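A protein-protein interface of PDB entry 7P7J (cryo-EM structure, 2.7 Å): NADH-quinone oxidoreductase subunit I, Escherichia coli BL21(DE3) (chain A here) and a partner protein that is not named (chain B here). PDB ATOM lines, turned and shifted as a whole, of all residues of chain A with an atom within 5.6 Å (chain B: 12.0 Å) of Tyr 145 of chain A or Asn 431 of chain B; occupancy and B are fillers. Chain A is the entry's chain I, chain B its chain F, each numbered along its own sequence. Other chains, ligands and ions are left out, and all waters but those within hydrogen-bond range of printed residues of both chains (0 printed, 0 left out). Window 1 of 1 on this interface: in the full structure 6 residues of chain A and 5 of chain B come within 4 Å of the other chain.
The guanidinium group of Arg 59 of chain A sits at hydrogen-bond distance from the backbone carbonyl oxygen of Tyr 145 of chain A (2.6 Å).
The side-chain hydroxyl (OH) of Tyr 145 of chain A sits at hydrogen-bond distance from the side-chain carboxylate (OE2) of Glu 106 of chain A (2.9 Å).
Among the printed residues, merely in contact across the chains: Glu 147 of chain A with Asn 431 of chain B (3.3 Å), Pro 146 of chain A with Asn 431 of chain B (3.4 Å), Tyr 145 of chain A with Gly 432 of chain B (3.6 Å), Tyr 145 of chain A with Ile 433 of chain B (3.6 Å) and Tyr 145 of chain A with Asn 431 of chain B (3.8 Å).
Of chain B, only Asn 431 (3.8 Å), Gly 432 (3.6 Å) and Ile 433 (3.6 Å) come within 4 Å of Tyr 145 of chain A.
Of chain A, only Tyr 145, Pro 146 and Glu 147 come within 4 Å of Asn 431 of chain B.
No residue of chain B comes within 4 Å of Pro 142 of chain A.
Of chain B, only Asn 431 (3.3 Å) comes within 4 Å of Glu 147 of chain A.
Of the printed residues of chain A, Gly 432 of chain B touches Tyr 145.
Of the printed residues of chain A, Ile 433 of chain B touches Tyr 145 (3.6 Å).
The nearest residue of chain A that does not touch Asn 431 of chain B is Lys 144 of chain A (4.3 Å).
Of the 12 printed residues of chain A, 3 touch a printed residue of chain B.
Hydrophobic or aromatic side chains of chain A within 4 Å of the printed part of chain B: Tyr 145 and Pro 146.
Hydrophobic or aromatic side chains of chain B within 4 Å of the printed part of chain A: Ile 433.
Among the printed residues, no Asp or Glu carboxylate lies within 4 Å of a Lys or Arg side-chain nitrogen of the other chain.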
ATOM      1  N   ARG A  59      27.108 -13.639  -9.847  1.00  0.00           N
ATOM      2  CA  ARG A  59      26.900 -14.227  -8.534  1.00  0.00           C
ATOM      3  C   ARG A  59      28.147 -14.222  -7.670  1.00  0.00           C
ATOM      4  O   ARG A  59      28.027 -14.338  -6.447  1.00  0.00           O
ATOM      5  CB  ARG A  59      26.394 -15.660  -8.672  1.00  0.00           C
ATOM      6  CG  ARG A  59      24.918 -15.745  -8.898  1.00  0.00           C
ATOM      7  CD  ARG A  59      24.315 -16.965  -8.271  1.00  0.00           C
ATOM      8  NE  ARG A  59      24.204 -18.073  -9.207  1.00  0.00           N
ATOM      9  CZ  ARG A  59      23.062 -18.666  -9.523  1.00  0.00           C
ATOM     10  NH1 ARG A  59      21.910 -18.264  -9.018  1.00  0.00           N
ATOM     11  NH2 ARG A  59      23.078 -19.695 -10.363  1.00  0.00           N
ATOM     12  N   GLU A 106      33.234 -25.813  -6.961  1.00  0.00           N
ATOM     13  CA  GLU A 106      31.779 -25.720  -6.990  1.00  0.00           C
ATOM     14  C   GLU A 106      31.183 -26.135  -5.655  1.00  0.00           C
ATOM     15  O   GLU A 106      30.216 -25.530  -5.181  1.00  0.00           O
ATOM     16  CB  GLU A 106      31.220 -26.585  -8.117  1.00  0.00           C
ATOM     17  CG  GLU A 106      29.715 -26.484  -8.275  1.00  0.00           C
ATOM     18  CD  GLU A 106      29.176 -27.362  -9.376  1.00  0.00           C
ATOM     19  OE1 GLU A 106      29.943 -27.719 -10.291  1.00  0.00           O
ATOM     20  OE2 GLU A 106      27.979 -27.699  -9.326  1.00  0.00           O
ATOM     21  N   THR A 112      26.962 -20.320  -5.285  1.00  0.00           N
ATOM     22  CA  THR A 112      26.764 -21.101  -6.515  1.00  0.00           C
ATOM     23  C   THR A 112      27.164 -20.313  -7.758  1.00  0.00           C
ATOM     24  O   THR A 112      26.539 -20.419  -8.814  1.00  0.00           O
ATOM     25  CB  THR A 112      25.329 -21.624  -6.651  1.00  0.00           C
ATOM     26  OG1 THR A 112      24.437 -20.536  -6.916  1.00  0.00           O
ATOM     27  CG2 THR A 112      24.893 -22.342  -5.396  1.00  0.00           C
ATOM     28  N   ILE A 114      30.524 -20.384  -9.135  1.00  0.00           N
ATOM     29  CA  ILE A 114      31.406 -21.239  -9.910  1.00  0.00           C
ATOM     30  C   ILE A 114      30.738 -22.601 -10.061  1.00  0.00           C
ATOM     31  O   ILE A 114      30.236 -23.175  -9.088  1.00  0.00           O
ATOM     32  CB  ILE A 114      32.803 -21.326  -9.261  1.00  0.00           C
ATOM     33  CG1 ILE A 114      33.741 -22.201 -10.064  1.00  0.00           C
ATOM     34  CG2 ILE A 114      32.767 -21.828  -7.843  1.00  0.00           C
ATOM     35  CD1 ILE A 114      35.187 -21.872  -9.844  1.00  0.00           C
ATOM     36  N   GLN A 115      30.644 -23.077 -11.301  1.00  0.00           N
ATOM     37  CA  GLN A 115      29.954 -24.325 -11.584  1.00  0.00           C
ATOM     38  C   GLN A 115      30.732 -25.115 -12.621  1.00  0.00           C
ATOM     39  O   GLN A 115      31.357 -24.547 -13.515  1.00  0.00           O
ATOM     40  CB  GLN A 115      28.525 -24.085 -12.095  1.00  0.00           C
ATOM     41  CG  GLN A 115      27.561 -23.521 -11.070  1.00  0.00           C
ATOM     42  CD  GLN A 115      26.235 -23.129 -11.676  1.00  0.00           C
ATOM     43  OE1 GLN A 115      25.850 -23.632 -12.727  1.00  0.00           O
ATOM     44  NE2 GLN A 115      25.536 -22.215 -11.028  1.00  0.00           N
ATOM     45  N   PRO A 142      21.969 -18.343 -14.913  1.00  0.00           N
ATOM     46  CA  PRO A 142      22.235 -18.943 -13.602  1.00  0.00           C
ATOM     47  C   PRO A 142      22.800 -20.353 -13.636  1.00  0.00           C
ATOM     48  O   PRO A 142      23.124 -20.885 -12.570  1.00  0.00           O
ATOM     49  CB  PRO A 142      20.852 -18.925 -12.946  1.00  0.00           C
ATOM     50  CG  PRO A 142      19.917 -19.071 -14.075  1.00  0.00           C
ATOM     51  CD  PRO A 142      20.535 -18.364 -15.246  1.00  0.00           C
ATOM     52  N   GLY A 143      22.926 -20.973 -14.804  1.00  0.00           N
ATOM     53  CA  GLY A 143      23.534 -22.293 -14.865  1.00  0.00           C
ATOM     54  C   GLY A 143      22.649 -23.364 -14.259  1.00  0.00           C
ATOM     55  O   GLY A 143      21.458 -23.469 -14.569  1.00  0.00           O
ATOM     56  N   LYS A 144      23.233 -24.174 -13.381  1.00  0.00           N
ATOM     57  CA  LYS A 144      22.551 -25.327 -12.811  1.00  0.00           C
ATOM     58  C   LYS A 144      21.700 -24.995 -11.594  1.00  0.00           C
ATOM     59  O   LYS A 144      20.888 -25.828 -11.186  1.00  0.00           O
ATOM     60  CB  LYS A 144      23.571 -26.404 -12.429  1.00  0.00           C
ATOM     61  CG  LYS A 144      24.393 -26.905 -13.594  1.00  0.00           C
ATOM     62  CD  LYS A 144      25.331 -28.013 -13.174  1.00  0.00           C
ATOM     63  CE  LYS A 144      26.299 -27.535 -12.118  1.00  0.00           C
ATOM     64  NZ  LYS A 144      27.344 -28.548 -11.831  1.00  0.00           N
ATOM     65  N   TYR A 145      21.857 -23.808 -11.010  1.00  0.00           N
ATOM     66  CA  TYR A 145      21.116 -23.400  -9.818  1.00  0.00           C
ATOM     67  C   TYR A 145      20.353 -22.131 -10.167  1.00  0.00           C
ATOM     68  O   TYR A 145      20.893 -21.019 -10.070  1.00  0.00           O
ATOM     69  CB  TYR A 145      22.058 -23.196  -8.636  1.00  0.00           C
ATOM     70  CG  TYR A 145      22.974 -24.374  -8.413  1.00  0.00           C
ATOM     71  CD1 TYR A 145      22.500 -25.547  -7.847  1.00  0.00           C
ATOM     72  CD2 TYR A 145      24.306 -24.323  -8.792  1.00  0.00           C
ATOM     73  CE1 TYR A 145      23.330 -26.628  -7.652  1.00  0.00           C
ATOM     74  CE2 TYR A 145      25.143 -25.398  -8.598  1.00  0.00           C
ATOM     75  CZ  TYR A 145      24.651 -26.547  -8.030  1.00  0.00           C
ATOM     76  OH  TYR A 145      25.484 -27.621  -7.840  1.00  0.00           O
ATOM     77  N   PRO A 146      19.091 -22.250 -10.563  1.00  0.00           N
ATOM     78  CA  PRO A 146      18.422 -21.142 -11.256  1.00  0.00           C
ATOM     79  C   PRO A 146      17.959 -19.983 -10.388  1.00  0.00           C
ATOM     80  O   PRO A 146      17.891 -18.855 -10.882  1.00  0.00           O
ATOM     81  CB  PRO A 146      17.228 -21.834 -11.918  1.00  0.00           C
ATOM     82  CG  PRO A 146      16.936 -22.981 -11.038  1.00  0.00           C
ATOM     83  CD  PRO A 146      18.255 -23.460 -10.522  1.00  0.00           C
ATOM     84  N   GLU A 147      17.626 -20.211  -9.119  1.00  0.00           N
ATOM     85  CA  GLU A 147      16.970 -19.174  -8.336  1.00  0.00           C
ATOM     86  C   GLU A 147      17.762 -18.659  -7.145  1.00  0.00           C
ATOM     87  O   GLU A 147      17.339 -17.669  -6.541  1.00  0.00           O
ATOM     88  CB  GLU A 147      15.600 -19.663  -7.842  1.00  0.00           C
ATOM     89  CG  GLU A 147      14.554 -19.761  -8.936  1.00  0.00           C
ATOM     90  CD  GLU A 147      13.994 -21.156  -9.087  1.00  0.00           C
ATOM     91  OE1 GLU A 147      14.047 -21.929  -8.109  1.00  0.00           O
ATOM     92  OE2 GLU A 147      13.499 -21.478 -10.187  1.00  0.00           O
ATOM     93  N   TYR A 148      18.878 -19.284  -6.779  1.00  0.00           N
ATOM     94  CA  TYR A 148      19.582 -18.860  -5.576  1.00  0.00           C
ATOM     95  C   TYR A 148      20.270 -17.520  -5.793  1.00  0.00           C
ATOM     96  O   TYR A 148      20.945 -17.307  -6.803  1.00  0.00           O
ATOM     97  CB  TYR A 148      20.605 -19.900  -5.132  1.00  0.00           C
ATOM     98  CG  TYR A 148      21.233 -19.536  -3.807  1.00  0.00           C
ATOM     99  CD1 TYR A 148      20.523 -19.673  -2.625  1.00  0.00           C
ATOM    100  CD2 TYR A 148      22.522 -19.025  -3.739  1.00  0.00           C
ATOM    101  CE1 TYR A 148      21.080 -19.328  -1.415  1.00  0.00           C
ATOM    102  CE2 TYR A 148      23.087 -18.674  -2.528  1.00  0.00           C
ATOM    103  CZ  TYR A 148      22.361 -18.829  -1.370  1.00  0.00           C
ATOM    104  OH  TYR A 148      22.915 -18.488  -0.162  1.00  0.00           O
ATOM    105  N   THR B 427      14.261 -24.613   6.552  1.00  0.00           N
ATOM    106  CA  THR B 427      14.865 -24.409   5.248  1.00  0.00           C
ATOM    107  C   THR B 427      13.783 -24.346   4.182  1.00  0.00           C
ATOM    108  O   THR B 427      12.731 -24.976   4.306  1.00  0.00           O
ATOM    109  CB  THR B 427      15.837 -25.546   4.895  1.00  0.00           C
ATOM    110  OG1 THR B 427      15.090 -26.702   4.500  1.00  0.00           O
ATOM    111  CG2 THR B 427      16.696 -25.913   6.083  1.00  0.00           C
ATOM    112  N   HIS B 428      14.048 -23.580   3.130  1.00  0.00           N
ATOM    113  CA  HIS B 428      13.249 -23.644   1.918  1.00  0.00           C
ATOM    114  C   HIS B 428      14.048 -24.348   0.832  1.00  0.00           C
ATOM    115  O   HIS B 428      15.281 -24.360   0.857  1.00  0.00           O
ATOM    116  CB  HIS B 428      12.797 -22.253   1.451  1.00  0.00           C
ATOM    117  CG  HIS B 428      13.913 -21.286   1.211  1.00  0.00           C
ATOM    118  ND1 HIS B 428      14.711 -21.330   0.088  1.00  0.00           N
ATOM    119  CD2 HIS B 428      14.341 -20.223   1.934  1.00  0.00           C
ATOM    120  CE1 HIS B 428      15.595 -20.349   0.140  1.00  0.00           C
ATOM    121  NE2 HIS B 428      15.392 -19.664   1.250  1.00  0.00           N
ATOM    122  N   LEU B 429      13.332 -24.958  -0.107  1.00  0.00           N
ATOM    123  CA  LEU B 429      13.977 -25.748  -1.147  1.00  0.00           C
ATOM    124  C   LEU B 429      14.724 -24.848  -2.119  1.00  0.00           C
ATOM    125  O   LEU B 429      14.184 -23.851  -2.605  1.00  0.00           O
ATOM    126  CB  LEU B 429      12.943 -26.583  -1.896  1.00  0.00           C
ATOM    127  CG  LEU B 429      12.176 -27.637  -1.098  1.00  0.00           C
ATOM    128  CD1 LEU B 429      11.334 -28.492  -2.030  1.00  0.00           C
ATOM    129  CD2 LEU B 429      13.128 -28.499  -0.283  1.00  0.00           C
ATOM    130  N   ILE B 430      15.971 -25.205  -2.402  1.00  0.00           N
ATOM    131  CA  ILE B 430      16.790 -24.513  -3.388  1.00  0.00           C
ATOM    132  C   ILE B 430      16.860 -25.408  -4.615  1.00  0.00           C
ATOM    133  O   ILE B 430      17.254 -26.576  -4.516  1.00  0.00           O
ATOM    134  CB  ILE B 430      18.188 -24.194  -2.842  1.00  0.00           C
ATOM    135  CG1 ILE B 430      18.068 -23.362  -1.567  1.00  0.00           C
ATOM    136  CG2 ILE B 430      19.011 -23.456  -3.881  1.00  0.00           C
ATOM    137  CD1 ILE B 430      19.376 -23.096  -0.892  1.00  0.00           C
ATOM    138  N   ASN B 431      16.464 -24.865  -5.762  1.00  0.00           N
ATOM    139  CA  ASN B 431      16.364 -25.661  -6.977  1.00  0.00           C
ATOM    140  C   ASN B 431      17.747 -26.074  -7.459  1.00  0.00           C
ATOM    141  O   ASN B 431      18.649 -25.242  -7.579  1.00  0.00           O
ATOM    142  CB  ASN B 431      15.637 -24.873  -8.062  1.00  0.00           C
ATOM    143  CG  ASN B 431      14.977 -25.767  -9.082  1.00  0.00           C
ATOM    144  OD1 ASN B 431      14.923 -26.985  -8.913  1.00  0.00           O
ATOM    145  ND2 ASN B 431      14.464 -25.169 -10.149  1.00  0.00           N
ATOM    146  N   GLY B 432      17.908 -27.363  -7.739  1.00  0.00           N
ATOM    147  CA  GLY B 432      19.179 -27.918  -8.142  1.00  0.00           C
ATOM    148  C   GLY B 432      19.971 -28.569  -7.030  1.00  0.00           C
ATOM    149  O   GLY B 432      20.947 -29.270  -7.320  1.00  0.00           O
ATOM    150  N   ILE B 433      19.588 -28.364  -5.773  1.00  0.00           N
ATOM    151  CA  ILE B 433      20.305 -28.919  -4.631  1.00  0.00           C
ATOM    152  C   ILE B 433      19.378 -29.878  -3.902  1.00  0.00           C
ATOM    153  O   ILE B 433      18.338 -29.465  -3.377  1.00  0.00           O
ATOM    154  CB  ILE B 433      20.807 -27.823  -3.682  1.00  0.00           C
ATOM    155  CG1 ILE B 433      21.714 -26.851  -4.433  1.00  0.00           C
ATOM    156  CG2 ILE B 433      21.539 -28.442  -2.509  1.00  0.00           C
ATOM    157  CD1 ILE B 433      22.306 -25.783  -3.563  1.00  0.00           C
ATOM    158  N   GLN B 434      19.757 -31.143  -3.863  1.00  0.00           N
ATOM    159  CA  GLN B 434      18.983 -32.136  -3.131  1.00  0.00           C
ATOM    160  C   GLN B 434      19.256 -32.003  -1.638  1.00  0.00           C
ATOM    161  O   GLN B 434      20.419 -31.996  -1.226  1.00  0.00           O
ATOM    162  CB  GLN B 434      19.326 -33.540  -3.601  1.00  0.00           C
ATOM    163  CG  GLN B 434      18.574 -33.969  -4.841  1.00  0.00           C
ATOM    164  CD  GLN B 434      19.234 -35.129  -5.542  1.00  0.00           C
ATOM    165  OE1 GLN B 434      20.398 -35.055  -5.927  1.00  0.00           O
ATOM    166  NE2 GLN B 434      18.492 -36.216  -5.712  1.00  0.00           N
ATOM    167  N   PRO B 435      18.225 -31.889  -0.807  1.00  0.00           N
ATOM    168  CA  PRO B 435      18.449 -31.731   0.632  1.00  0.00           C
ATOM    169  C   PRO B 435      18.923 -33.019   1.286  1.00  0.00           C
ATOM    170  O   PRO B 435      18.779 -34.120   0.750  1.00  0.00           O
ATOM    171  CB  PRO B 435      17.071 -31.317   1.157  1.00  0.00           C
ATOM    172  CG  PRO B 435      16.120 -31.899   0.178  1.00  0.00           C
ATOM    173  CD  PRO B 435      16.797 -31.813  -1.155  1.00  0.00           C
ATOM    174  N   ASN B 436      19.512 -32.858   2.468  1.00  0.00           N
ATOM    175  CA  ASN B 436      19.951 -33.978   3.297  1.00  0.00           C
ATOM    176  C   ASN B 436      18.791 -34.367   4.204  1.00  0.00           C
ATOM    177  O   ASN B 436      18.580 -33.764   5.258  1.00  0.00           O
ATOM    178  CB  ASN B 436      21.187 -33.596   4.101  1.00  0.00           C
ATOM    179  CG  ASN B 436      21.966 -34.797   4.585  1.00  0.00           C
ATOM    180  OD1 ASN B 436      22.022 -35.822   3.914  1.00  0.00           O
ATOM    181  ND2 ASN B 436      22.576 -34.674   5.754  1.00  0.00           N
